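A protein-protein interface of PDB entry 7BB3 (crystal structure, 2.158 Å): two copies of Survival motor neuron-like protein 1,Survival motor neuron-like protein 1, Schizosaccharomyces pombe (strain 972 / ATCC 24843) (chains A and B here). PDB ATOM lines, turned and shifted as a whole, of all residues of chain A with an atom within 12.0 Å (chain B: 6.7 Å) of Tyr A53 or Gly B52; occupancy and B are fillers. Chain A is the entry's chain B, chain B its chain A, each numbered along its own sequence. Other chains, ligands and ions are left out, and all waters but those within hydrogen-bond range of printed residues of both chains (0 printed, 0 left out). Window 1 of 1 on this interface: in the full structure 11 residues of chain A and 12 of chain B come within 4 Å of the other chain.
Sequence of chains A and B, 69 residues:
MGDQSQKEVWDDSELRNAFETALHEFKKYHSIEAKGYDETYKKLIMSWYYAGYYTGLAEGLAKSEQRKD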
ATOM      1  N   LEU A  44       6.499  -4.404 -10.312  1.00  0.00           N
ATOM      2  CA  LEU A  44       7.146  -5.710 -10.347  1.00  0.00           C
ATOM      3  C   LEU A  44       6.133  -6.810 -10.604  1.00  0.00           C
ATOM      4  O   LEU A  44       6.361  -7.704 -11.429  1.00  0.00           O
ATOM      5  CB  LEU A  44       7.876  -5.960  -9.029  1.00  0.00           C
ATOM      6  CG  LEU A  44       8.550  -7.322  -8.874  1.00  0.00           C
ATOM      7  CD1 LEU A  44       9.646  -7.478  -9.911  1.00  0.00           C
ATOM      8  CD2 LEU A  44       9.097  -7.480  -7.467  1.00  0.00           C
ATOM      9  N   ILE A  45       4.995  -6.755  -9.914  1.00  0.00           N
ATOM     10  CA  ILE A  45       3.988  -7.797 -10.039  1.00  0.00           C
ATOM     11  C   ILE A  45       3.357  -7.767 -11.427  1.00  0.00           C
ATOM     12  O   ILE A  45       3.186  -8.808 -12.068  1.00  0.00           O
ATOM     13  CB  ILE A  45       2.935  -7.645  -8.927  1.00  0.00           C
ATOM     14  CG1 ILE A  45       3.531  -8.094  -7.589  1.00  0.00           C
ATOM     15  CG2 ILE A  45       1.683  -8.432  -9.259  1.00  0.00           C
ATOM     16  CD1 ILE A  45       3.705  -9.592  -7.475  1.00  0.00           C
ATOM     17  N   MET A  46       3.002  -6.575 -11.911  1.00  0.00           N
ATOM     18  CA  MET A  46       2.411  -6.490 -13.243  1.00  0.00           C
ATOM     19  C   MET A  46       3.393  -6.964 -14.305  1.00  0.00           C
ATOM     20  O   MET A  46       3.000  -7.619 -15.280  1.00  0.00           O
ATOM     21  CB  MET A  46       1.958  -5.057 -13.524  1.00  0.00           C
ATOM     22  CG  MET A  46       0.795  -4.597 -12.653  1.00  0.00           C
ATOM     23  SD  MET A  46       0.261  -2.900 -12.968  1.00  0.00           S
ATOM     24  CE  MET A  46       1.528  -1.966 -12.111  1.00  0.00           C
ATOM     25  N   SER A  47       4.681  -6.662 -14.126  1.00  0.00           N
ATOM     26  CA  SER A  47       5.681  -7.060 -15.112  1.00  0.00           C
ATOM     27  C   SER A  47       5.742  -8.576 -15.259  1.00  0.00           C
ATOM     28  O   SER A  47       5.794  -9.100 -16.377  1.00  0.00           O
ATOM     29  CB  SER A  47       7.050  -6.505 -14.725  1.00  0.00           C
ATOM     30  OG  SER A  47       7.101  -5.103 -14.922  1.00  0.00           O
ATOM     31  N   TRP A  48       5.748  -9.302 -14.137  1.00  0.00           N
ATOM     32  CA  TRP A  48       5.836 -10.758 -14.224  1.00  0.00           C
ATOM     33  C   TRP A  48       4.548 -11.357 -14.775  1.00  0.00           C
ATOM     34  O   TRP A  48       4.592 -12.320 -15.549  1.00  0.00           O
ATOM     35  CB  TRP A  48       6.184 -11.356 -12.860  1.00  0.00           C
ATOM     36  CG  TRP A  48       7.664 -11.312 -12.578  1.00  0.00           C
ATOM     37  CD1 TRP A  48       8.312 -10.464 -11.727  1.00  0.00           C
ATOM     38  CD2 TRP A  48       8.679 -12.138 -13.169  1.00  0.00           C
ATOM     39  NE1 TRP A  48       9.663 -10.714 -11.745  1.00  0.00           N
ATOM     40  CE2 TRP A  48       9.915 -11.737 -12.621  1.00  0.00           C
ATOM     41  CE3 TRP A  48       8.662 -13.179 -14.103  1.00  0.00           C
ATOM     42  CZ2 TRP A  48      11.121 -12.340 -12.977  1.00  0.00           C
ATOM     43  CZ3 TRP A  48       9.862 -13.776 -14.454  1.00  0.00           C
ATOM     44  CH2 TRP A  48      11.073 -13.355 -13.892  1.00  0.00           C
ATOM     45  N   TYR A  49       3.392 -10.796 -14.406  1.00  0.00           N
ATOM     46  CA  TYR A  49       2.154 -11.207 -15.058  1.00  0.00           C
ATOM     47  C   TYR A  49       2.297 -11.120 -16.575  1.00  0.00           C
ATOM     48  O   TYR A  49       1.987 -12.070 -17.301  1.00  0.00           O
ATOM     49  CB  TYR A  49       0.977 -10.345 -14.590  1.00  0.00           C
ATOM     50  CG  TYR A  49      -0.307 -10.630 -15.351  1.00  0.00           C
ATOM     51  CD1 TYR A  49      -1.037 -11.785 -15.109  1.00  0.00           C
ATOM     52  CD2 TYR A  49      -0.784  -9.747 -16.315  1.00  0.00           C
ATOM     53  CE1 TYR A  49      -2.205 -12.054 -15.800  1.00  0.00           C
ATOM     54  CE2 TYR A  49      -1.952 -10.009 -17.012  1.00  0.00           C
ATOM     55  CZ  TYR A  49      -2.659 -11.165 -16.751  1.00  0.00           C
ATOM     56  OH  TYR A  49      -3.821 -11.431 -17.440  1.00  0.00           O
ATOM     57  N   TYR A  50       2.789  -9.980 -17.067  1.00  0.00           N
ATOM     58  CA  TYR A  50       2.828  -9.752 -18.508  1.00  0.00           C
ATOM     59  C   TYR A  50       3.862 -10.640 -19.192  1.00  0.00           C
ATOM     60  O   TYR A  50       3.601 -11.177 -20.275  1.00  0.00           O
ATOM     61  CB  TYR A  50       3.100  -8.275 -18.786  1.00  0.00           C
ATOM     62  CG  TYR A  50       1.872  -7.411 -18.621  1.00  0.00           C
ATOM     63  CD1 TYR A  50       0.680  -7.740 -19.254  1.00  0.00           C
ATOM     64  CD2 TYR A  50       1.896  -6.276 -17.823  1.00  0.00           C
ATOM     65  CE1 TYR A  50      -0.447  -6.964 -19.107  1.00  0.00           C
ATOM     66  CE2 TYR A  50       0.767  -5.490 -17.669  1.00  0.00           C
ATOM     67  CZ  TYR A  50      -0.400  -5.839 -18.314  1.00  0.00           C
ATOM     68  OH  TYR A  50      -1.527  -5.066 -18.168  1.00  0.00           O
ATOM     69  N   ALA A  51       5.043 -10.803 -18.590  1.00  0.00           N
ATOM     70  CA  ALA A  51       6.002 -11.755 -19.143  1.00  0.00           C
ATOM     71  C   ALA A  51       5.353 -13.119 -19.326  1.00  0.00           C
ATOM     72  O   ALA A  51       5.510 -13.759 -20.374  1.00  0.00           O
ATOM     73  CB  ALA A  51       7.227 -11.864 -18.235  1.00  0.00           C
ATOM     74  N   GLY A  52       4.603 -13.573 -18.322  1.00  0.00           N
ATOM     75  CA  GLY A  52       3.886 -14.828 -18.458  1.00  0.00           C
ATOM     76  C   GLY A  52       2.839 -14.775 -19.551  1.00  0.00           C
ATOM     77  O   GLY A  52       2.746 -15.681 -20.384  1.00  0.00           O
ATOM     78  N   TYR A  53       2.042 -13.705 -19.571  1.00  0.00           N
ATOM     79  CA  TYR A  53       0.998 -13.577 -20.580  1.00  0.00           C
ATOM     80  C   TYR A  53       1.566 -13.766 -21.984  1.00  0.00           C
ATOM     81  O   TYR A  53       1.119 -14.637 -22.739  1.00  0.00           O
ATOM     82  CB  TYR A  53       0.313 -12.213 -20.465  1.00  0.00           C
ATOM     83  CG  TYR A  53      -0.753 -12.003 -21.517  1.00  0.00           C
ATOM     84  CD1 TYR A  53      -1.981 -12.641 -21.422  1.00  0.00           C
ATOM     85  CD2 TYR A  53      -0.530 -11.171 -22.607  1.00  0.00           C
ATOM     86  CE1 TYR A  53      -2.956 -12.460 -22.381  1.00  0.00           C
ATOM     87  CE2 TYR A  53      -1.501 -10.983 -23.571  1.00  0.00           C
ATOM     88  CZ  TYR A  53      -2.711 -11.630 -23.453  1.00  0.00           C
ATOM     89  OH  TYR A  53      -3.682 -11.446 -24.412  1.00  0.00           O
ATOM     90  N   TYR A  54       2.563 -12.959 -22.351  1.00  0.00           N
ATOM     91  CA  TYR A  54       3.056 -12.999 -23.724  1.00  0.00           C
ATOM     92  C   TYR A  54       3.832 -14.273 -24.014  1.00  0.00           C
ATOM     93  O   TYR A  54       3.863 -14.725 -25.165  1.00  0.00           O
ATOM     94  CB  TYR A  54       3.907 -11.766 -24.009  1.00  0.00           C
ATOM     95  CG  TYR A  54       3.064 -10.521 -24.100  1.00  0.00           C
ATOM     96  CD1 TYR A  54       2.189 -10.334 -25.161  1.00  0.00           C
ATOM     97  CD2 TYR A  54       3.119  -9.547 -23.117  1.00  0.00           C
ATOM     98  CE1 TYR A  54       1.403  -9.207 -25.246  1.00  0.00           C
ATOM     99  CE2 TYR A  54       2.337  -8.414 -23.194  1.00  0.00           C
ATOM    100  CZ  TYR A  54       1.479  -8.251 -24.261  1.00  0.00           C
ATOM    101  OH  TYR A  54       0.697  -7.124 -24.342  1.00  0.00           O
ATOM    102  N   THR A  55       4.457 -14.873 -23.000  1.00  0.00           N
ATOM    103  CA  THR A  55       5.092 -16.166 -23.216  1.00  0.00           C
ATOM    104  C   THR A  55       4.052 -17.235 -23.516  1.00  0.00           C
ATOM    105  O   THR A  55       4.258 -18.083 -24.394  1.00  0.00           O
ATOM    106  CB  THR A  55       5.920 -16.569 -21.997  1.00  0.00           C
ATOM    107  OG1 THR A  55       6.871 -15.541 -21.700  1.00  0.00           O
ATOM    108  CG2 THR A  55       6.657 -17.876 -22.268  1.00  0.00           C
ATOM    109  N   GLY A  56       2.933 -17.220 -22.789  1.00  0.00           N
ATOM    110  CA  GLY A  56       1.917 -18.233 -23.021  1.00  0.00           C
ATOM    111  C   GLY A  56       1.195 -18.024 -24.335  1.00  0.00           C
ATOM    112  O   GLY A  56       0.903 -18.984 -25.053  1.00  0.00           O
ATOM    113  N   LEU A  57       0.922 -16.765 -24.680  1.00  0.00           N
ATOM    114  CA  LEU A  57       0.289 -16.447 -25.952  1.00  0.00           C
ATOM    115  C   LEU A  57       1.115 -16.968 -27.118  1.00  0.00           C
ATOM    116  O   LEU A  57       0.601 -17.682 -27.985  1.00  0.00           O
ATOM    117  CB  LEU A  57       0.098 -14.935 -26.051  1.00  0.00           C
ATOM    118  CG  LEU A  57      -0.738 -14.399 -27.208  1.00  0.00           C
ATOM    119  CD1 LEU A  57      -2.132 -14.995 -27.186  1.00  0.00           C
ATOM    120  CD2 LEU A  57      -0.802 -12.880 -27.147  1.00  0.00           C
ATOM    121  N   ALA A  58       2.406 -16.627 -27.152  1.00  0.00           N
ATOM    122  CA  ALA A  58       3.259 -17.071 -28.251  1.00  0.00           C
ATOM    123  C   ALA A  58       3.261 -18.589 -28.371  1.00  0.00           C
ATOM    124  O   ALA A  58       3.170 -19.131 -29.480  1.00  0.00           O
ATOM    125  CB  ALA A  58       4.682 -16.547 -28.054  1.00  0.00           C
ATOM    126  N   GLU A  59       3.370 -19.298 -27.244  1.00  0.00           N
ATOM    127  CA  GLU A  59       3.311 -20.753 -27.289  1.00  0.00           C
ATOM    128  C   GLU A  59       1.965 -21.233 -27.815  1.00  0.00           C
ATOM    129  O   GLU A  59       1.897 -22.251 -28.516  1.00  0.00           O
ATOM    130  CB  GLU A  59       3.567 -21.337 -25.902  1.00  0.00           C
ATOM    131  CG  GLU A  59       4.944 -21.023 -25.350  1.00  0.00           C
ATOM    132  CD  GLU A  59       5.186 -21.641 -23.987  1.00  0.00           C
ATOM    133  OE1 GLU A  59       4.325 -22.421 -23.523  1.00  0.00           O
ATOM    134  OE2 GLU A  59       6.235 -21.342 -23.379  1.00  0.00           O
ATOM    135  N   GLY A  60       0.888 -20.516 -27.484  1.00  0.00           N
ATOM    136  CA  GLY A  60      -0.428 -20.949 -27.926  1.00  0.00           C
ATOM    137  C   GLY A  60      -0.646 -20.711 -29.408  1.00  0.00           C
ATOM    138  O   GLY A  60      -1.271 -21.526 -30.091  1.00  0.00           O
ATOM    139  N   LEU A  61      -0.128 -19.598 -29.926  1.00  0.00           N
ATOM    140  CA  LEU A  61      -0.228 -19.331 -31.354  1.00  0.00           C
ATOM    141  C   LEU A  61       0.613 -20.313 -32.156  1.00  0.00           C
ATOM    142  O   LEU A  61       0.191 -20.771 -33.224  1.00  0.00           O
ATOM    143  CB  LEU A  61       0.211 -17.899 -31.642  1.00  0.00           C
ATOM    144  CG  LEU A  61      -0.673 -16.807 -31.044  1.00  0.00           C
ATOM    145  CD1 LEU A  61      -0.061 -15.443 -31.308  1.00  0.00           C
ATOM    146  CD2 LEU A  61      -2.077 -16.897 -31.611  1.00  0.00           C
ATOM    147  N   ALA A  62       1.807 -20.644 -31.661  1.00  0.00           N
ATOM    148  CA  ALA A  62       2.682 -21.551 -32.395  1.00  0.00           C
ATOM    149  C   ALA A  62       2.002 -22.891 -32.647  1.00  0.00           C
ATOM    150  O   ALA A  62       2.196 -23.508 -33.700  1.00  0.00           O
ATOM    151  CB  ALA A  62       3.991 -21.748 -31.632  1.00  0.00           C
ATOM    152  N   SER B  47       3.065 -16.622  -8.702  1.00  0.00           N
ATOM    153  CA  SER B  47       1.648 -16.889  -8.930  1.00  0.00           C
ATOM    154  C   SER B  47       1.085 -15.969 -10.001  1.00  0.00           C
ATOM    155  O   SER B  47       0.272 -16.392 -10.833  1.00  0.00           O
ATOM    156  CB  SER B  47       0.872 -16.732  -7.624  1.00  0.00           C
ATOM    157  OG  SER B  47       1.258 -17.724  -6.689  1.00  0.00           O
ATOM    158  N   TRP B  48       1.509 -14.705 -10.003  1.00  0.00           N
ATOM    159  CA  TRP B  48       1.082 -13.788 -11.050  1.00  0.00           C
ATOM    160  C   TRP B  48       1.716 -14.135 -12.385  1.00  0.00           C
ATOM    161  O   TRP B  48       1.103 -13.912 -13.436  1.00  0.00           O
ATOM    162  CB  TRP B  48       1.407 -12.357 -10.641  1.00  0.00           C
ATOM    163  CG  TRP B  48       0.349 -11.822  -9.760  1.00  0.00           C
ATOM    164  CD1 TRP B  48       0.416 -11.623  -8.413  1.00  0.00           C
ATOM    165  CD2 TRP B  48      -0.972 -11.453 -10.157  1.00  0.00           C
ATOM    166  NE1 TRP B  48      -0.782 -11.136  -7.950  1.00  0.00           N
ATOM    167  CE2 TRP B  48      -1.651 -11.023  -9.003  1.00  0.00           C
ATOM    168  CE3 TRP B  48      -1.646 -11.439 -11.383  1.00  0.00           C
ATOM    169  CZ2 TRP B  48      -2.971 -10.580  -9.038  1.00  0.00           C
ATOM    170  CZ3 TRP B  48      -2.954 -10.999 -11.415  1.00  0.00           C
ATOM    171  CH2 TRP B  48      -3.604 -10.577 -10.251  1.00  0.00           C
ATOM    172  N   TYR B  49       2.919 -14.703 -12.371  1.00  0.00           N
ATOM    173  CA  TYR B  49       3.529 -15.141 -13.619  1.00  0.00           C
ATOM    174  C   TYR B  49       2.725 -16.271 -14.254  1.00  0.00           C
ATOM    175  O   TYR B  49       2.455 -16.260 -15.462  1.00  0.00           O
ATOM    176  CB  TYR B  49       4.968 -15.592 -13.378  1.00  0.00           C
ATOM    177  CG  TYR B  49       5.574 -16.234 -14.601  1.00  0.00           C
ATOM    178  CD1 TYR B  49       6.138 -15.457 -15.601  1.00  0.00           C
ATOM    179  CD2 TYR B  49       5.555 -17.612 -14.770  1.00  0.00           C
ATOM    180  CE1 TYR B  49       6.681 -16.030 -16.724  1.00  0.00           C
ATOM    181  CE2 TYR B  49       6.096 -18.197 -15.898  1.00  0.00           C
ATOM    182  CZ  TYR B  49       6.658 -17.397 -16.870  1.00  0.00           C
ATOM    183  OH  TYR B  49       7.207 -17.949 -17.999  1.00  0.00           O
ATOM    184  N   TYR B  50       2.348 -17.272 -13.456  1.00  0.00           N
ATOM    185  CA  TYR B  50       1.648 -18.424 -14.012  1.00  0.00           C
ATOM    186  C   TYR B  50       0.216 -18.085 -14.395  1.00  0.00           C
ATOM    187  O   TYR B  50      -0.301 -18.625 -15.380  1.00  0.00           O
ATOM    188  CB  TYR B  50       1.686 -19.586 -13.020  1.00  0.00           C
ATOM    189  CG  TYR B  50       3.027 -20.283 -13.000  1.00  0.00           C
ATOM    190  CD1 TYR B  50       3.496 -20.947 -14.125  1.00  0.00           C
ATOM    191  CD2 TYR B  50       3.831 -20.269 -11.867  1.00  0.00           C
ATOM    192  CE1 TYR B  50       4.719 -21.577 -14.126  1.00  0.00           C
ATOM    193  CE2 TYR B  50       5.060 -20.902 -11.858  1.00  0.00           C
ATOM    194  CZ  TYR B  50       5.498 -21.554 -12.992  1.00  0.00           C
ATOM    195  OH  TYR B  50       6.719 -22.187 -12.995  1.00  0.00           O
ATOM    196  N   ALA B  51      -0.439 -17.200 -13.643  1.00  0.00           N
ATOM    197  CA  ALA B  51      -1.770 -16.756 -14.039  1.00  0.00           C
ATOM    198  C   ALA B  51      -1.728 -16.118 -15.422  1.00  0.00           C
ATOM    199  O   ALA B  51      -2.561 -16.416 -16.285  1.00  0.00           O
ATOM    200  CB  ALA B  51      -2.326 -15.780 -13.005  1.00  0.00           C
ATOM    201  N   GLY B  52      -0.746 -15.245 -15.654  1.00  0.00           N
ATOM    202  CA  GLY B  52      -0.573 -14.687 -16.981  1.00  0.00           C
ATOM    203  C   GLY B  52      -0.261 -15.746 -18.021  1.00  0.00           C
ATOM    204  O   GLY B  52      -0.790 -15.709 -19.133  1.00  0.00           O
ATOM    205  N   TYR B  53       0.588 -16.713 -17.667  1.00  0.00           N
ATOM    206  CA  TYR B  53       1.034 -17.703 -18.644  1.00  0.00           C
ATOM    207  C   TYR B  53      -0.132 -18.542 -19.152  1.00  0.00           C
ATOM    208  O   TYR B  53      -0.315 -18.708 -20.364  1.00  0.00           O
ATOM    209  CB  TYR B  53       2.115 -18.598 -18.030  1.00  0.00           C
ATOM    210  CG  TYR B  53       2.477 -19.793 -18.886  1.00  0.00           C
ATOM    211  CD1 TYR B  53       3.362 -19.670 -19.950  1.00  0.00           C
ATOM    212  CD2 TYR B  53       1.930 -21.045 -18.632  1.00  0.00           C
ATOM    213  CE1 TYR B  53       3.688 -20.758 -20.739  1.00  0.00           C
ATOM    214  CE2 TYR B  53       2.255 -22.141 -19.414  1.00  0.00           C
ATOM    215  CZ  TYR B  53       3.135 -21.992 -20.462  1.00  0.00           C
ATOM    216  OH  TYR B  53       3.456 -23.082 -21.240  1.00  0.00           O
ATOM    217  N   TYR B  54      -0.932 -19.090 -18.236  1.00  0.00           N
ATOM    218  CA  TYR B  54      -2.045 -19.937 -18.649  1.00  0.00           C
ATOM    219  C   TYR B  54      -3.173 -19.116 -19.258  1.00  0.00           C
ATOM    220  O   TYR B  54      -3.921 -19.626 -20.101  1.00  0.00           O
ATOM    221  CB  TYR B  54      -2.523 -20.764 -17.458  1.00  0.00           C
ATOM    222  CG  TYR B  54      -1.528 -21.841 -17.080  1.00  0.00           C
ATOM    223  CD1 TYR B  54      -1.329 -22.940 -17.903  1.00  0.00           C
ATOM    224  CD2 TYR B  54      -0.779 -21.754 -15.913  1.00  0.00           C
ATOM    225  CE1 TYR B  54      -0.420 -23.926 -17.576  1.00  0.00           C
ATOM    226  CE2 TYR B  54       0.133 -22.739 -15.575  1.00  0.00           C
ATOM    227  CZ  TYR B  54       0.309 -23.822 -16.413  1.00  0.00           C
ATOM    228  OH  TYR B  54       1.215 -24.808 -16.090  1.00  0.00           O
ATOM    229  N   THR B  55      -3.295 -17.847 -18.869  1.00  0.00           N
ATOM    230  CA  THR B  55      -4.214 -16.946 -19.558  1.00  0.00           C
ATOM    231  C   THR B  55      -3.788 -16.748 -21.008  1.00  0.00           C
ATOM    232  O   THR B  55      -4.582 -16.947 -21.935  1.00  0.00           O
ATOM    233  CB  THR B  55      -4.272 -15.604 -18.829  1.00  0.00           C
ATOM    234  OG1 THR B  55      -4.649 -15.817 -17.465  1.00  0.00           O
ATOM    235  CG2 THR B  55      -5.274 -14.669 -19.493  1.00  0.00           C
ATOM    236  N   GLY B  56      -2.532 -16.356 -21.223  1.00  0.00           N
ATOM    237  CA  GLY B  56      -2.050 -16.197 -22.585  1.00  0.00           C
ATOM    238  C   GLY B  56      -2.143 -17.478 -23.387  1.00  0.00           C
ATOM    239  O   GLY B  56      -2.540 -17.464 -24.554  1.00  0.00           O
ATOM    240  N   LEU B  57      -1.797 -18.608 -22.766  1.00  0.00           N
ATOM    241  CA  LEU B  57      -1.783 -19.880 -23.478  1.00  0.00           C
ATOM    242  C   LEU B  57      -3.173 -20.260 -23.969  1.00  0.00           C
ATOM    243  O   LEU B  57      -3.331 -20.717 -25.107  1.00  0.00           O
ATOM    244  CB  LEU B  57      -1.219 -20.963 -22.563  1.00  0.00           C
ATOM    245  CG  LEU B  57      -1.131 -22.396 -23.081  1.00  0.00           C
ATOM    246  CD1 LEU B  57      -0.151 -22.531 -24.224  1.00  0.00           C
ATOM    247  CD2 LEU B  57      -0.740 -23.308 -21.919  1.00  0.00           C
ATOM    248  N   GLU B  59      -5.720 -18.180 -24.569  1.00  0.00           N
ATOM    249  CA  GLU B  59      -6.038 -17.250 -25.647  1.00  0.00           C
ATOM    250  C   GLU B  59      -5.350 -17.656 -26.945  1.00  0.00           C
ATOM    251  O   GLU B  59      -5.928 -17.529 -28.032  1.00  0.00           O
ATOM    252  CB  GLU B  59      -5.627 -15.829 -25.265  1.00  0.00           C
ATOM    253  CG  GLU B  59      -6.403 -15.234 -24.109  1.00  0.00           C
ATOM    254  CD  GLU B  59      -6.192 -13.735 -23.981  1.00  0.00           C
ATOM    255  OE1 GLU B  59      -5.489 -13.151 -24.833  1.00  0.00           O
ATOM    256  OE2 GLU B  59      -6.735 -13.140 -23.026  1.00  0.00           O
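O of Gly B52 lies close to N of Tyr A53, at 3.5 Å. The side-chain hydroxyl of Tyr B53 lies within hydrogen-bond range of the side-chain carboxylate of Glu A59 (2.5 Å). The side-chain carboxylate (OE1) of Glu B59 is in hydrogen-bond range of the side-chain hydroxyl (OH) of Tyr A53 (2.5 Å).
Among the printed residues, merely in contact across the chains: Ile A45 with Trp B48 (3.5 Å), Trp A48 with Tyr B49 (3.5 Å), Tyr A49 with Trp B48 (3.3 Å), Tyr A49 with Gly B52 (3.3 Å), Gly A52 with Tyr B49 (3.5 Å), Gly A52 with Gly B52 (3.6 Å), Gly A52 with Tyr B53 (3.2 Å), Tyr A53 with Tyr B53 (3.8 Å), Tyr A53 with Gly B56 (3.5 Å), Gly A56 with Tyr B53 (3.5 Å), Gly A56 with Gly B56 (3.5 Å), Gly A56 with Leu B57 (3.2 Å), Leu A57 with Gly B56 (3.3 Å), Leu A57 with Leu B57 (3.8 Å) and Gly A60 with Leu B57 (3.97 Å).
Printed residues of chain B within 4 Å of Tyr A53: Gly B52 (3.1 Å), Tyr B53 (3.8 Å), Gly B56 (3.5 Å) and Glu B59 (2.5 Å). Gly B52 touches just these residues of chain A: Tyr A49 (3.3 Å), Gly A52 (3.6 Å) and Tyr A53 (3.1 Å). Tyr B49 touches just these residues of chain A: Trp A48 and Gly A52. No residue of chain A comes within 4 Å of Thr B55. Glu B59 touches one residue of chain A. Printed residues of chain A within 4 Å of Tyr B53: Gly A52 (3.2 Å), Tyr A53 (3.8 Å), Gly A56 (3.5 Å) and Glu A59 (2.5 Å). Of the printed residues of chain A, Trp B48 touches Ile A45 (3.5 Å) and Tyr A49 (3.3 Å). Of the printed residues of chain B, Ile A45 touches Trp B48. Thr A55 touches none of the printed residues of chain B.
Hydrophobic or aromatic side chains of chain B that line the printed part of chain A: Trp B48, Tyr B49, Tyr B53 and Leu B57. Along chain B the printed residues that touch a printed residue of chain A span positions 48 to 59. Printed residues of chain A that touch a printed residue of chain B: Ile A45, Trp A48, Tyr A49, Gly A52, Tyr A53, Gly A56, Leu A57, Glu A59 and Gly A60.
Trp A48 touches Tyr B49, and with the chains exchanged Tyr A49 touches Trp B48. Tyr A49 touches Gly B52, and with the chains exchanged Gly A52 touches Tyr B49. Gly A52 touches Tyr B53, and with the chains exchanged Tyr A53 touches Gly B52. Tyr A53 touches its own counterpart, Tyr B53. Positions printed for both chains: 47, 48, 49, 50, 51, 52, 53, 54, 55, 56, 57 and 59. Of the 18 pairs that touch across the chains among the printed residues, 16 have their exchanged pair printed and touching as well.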
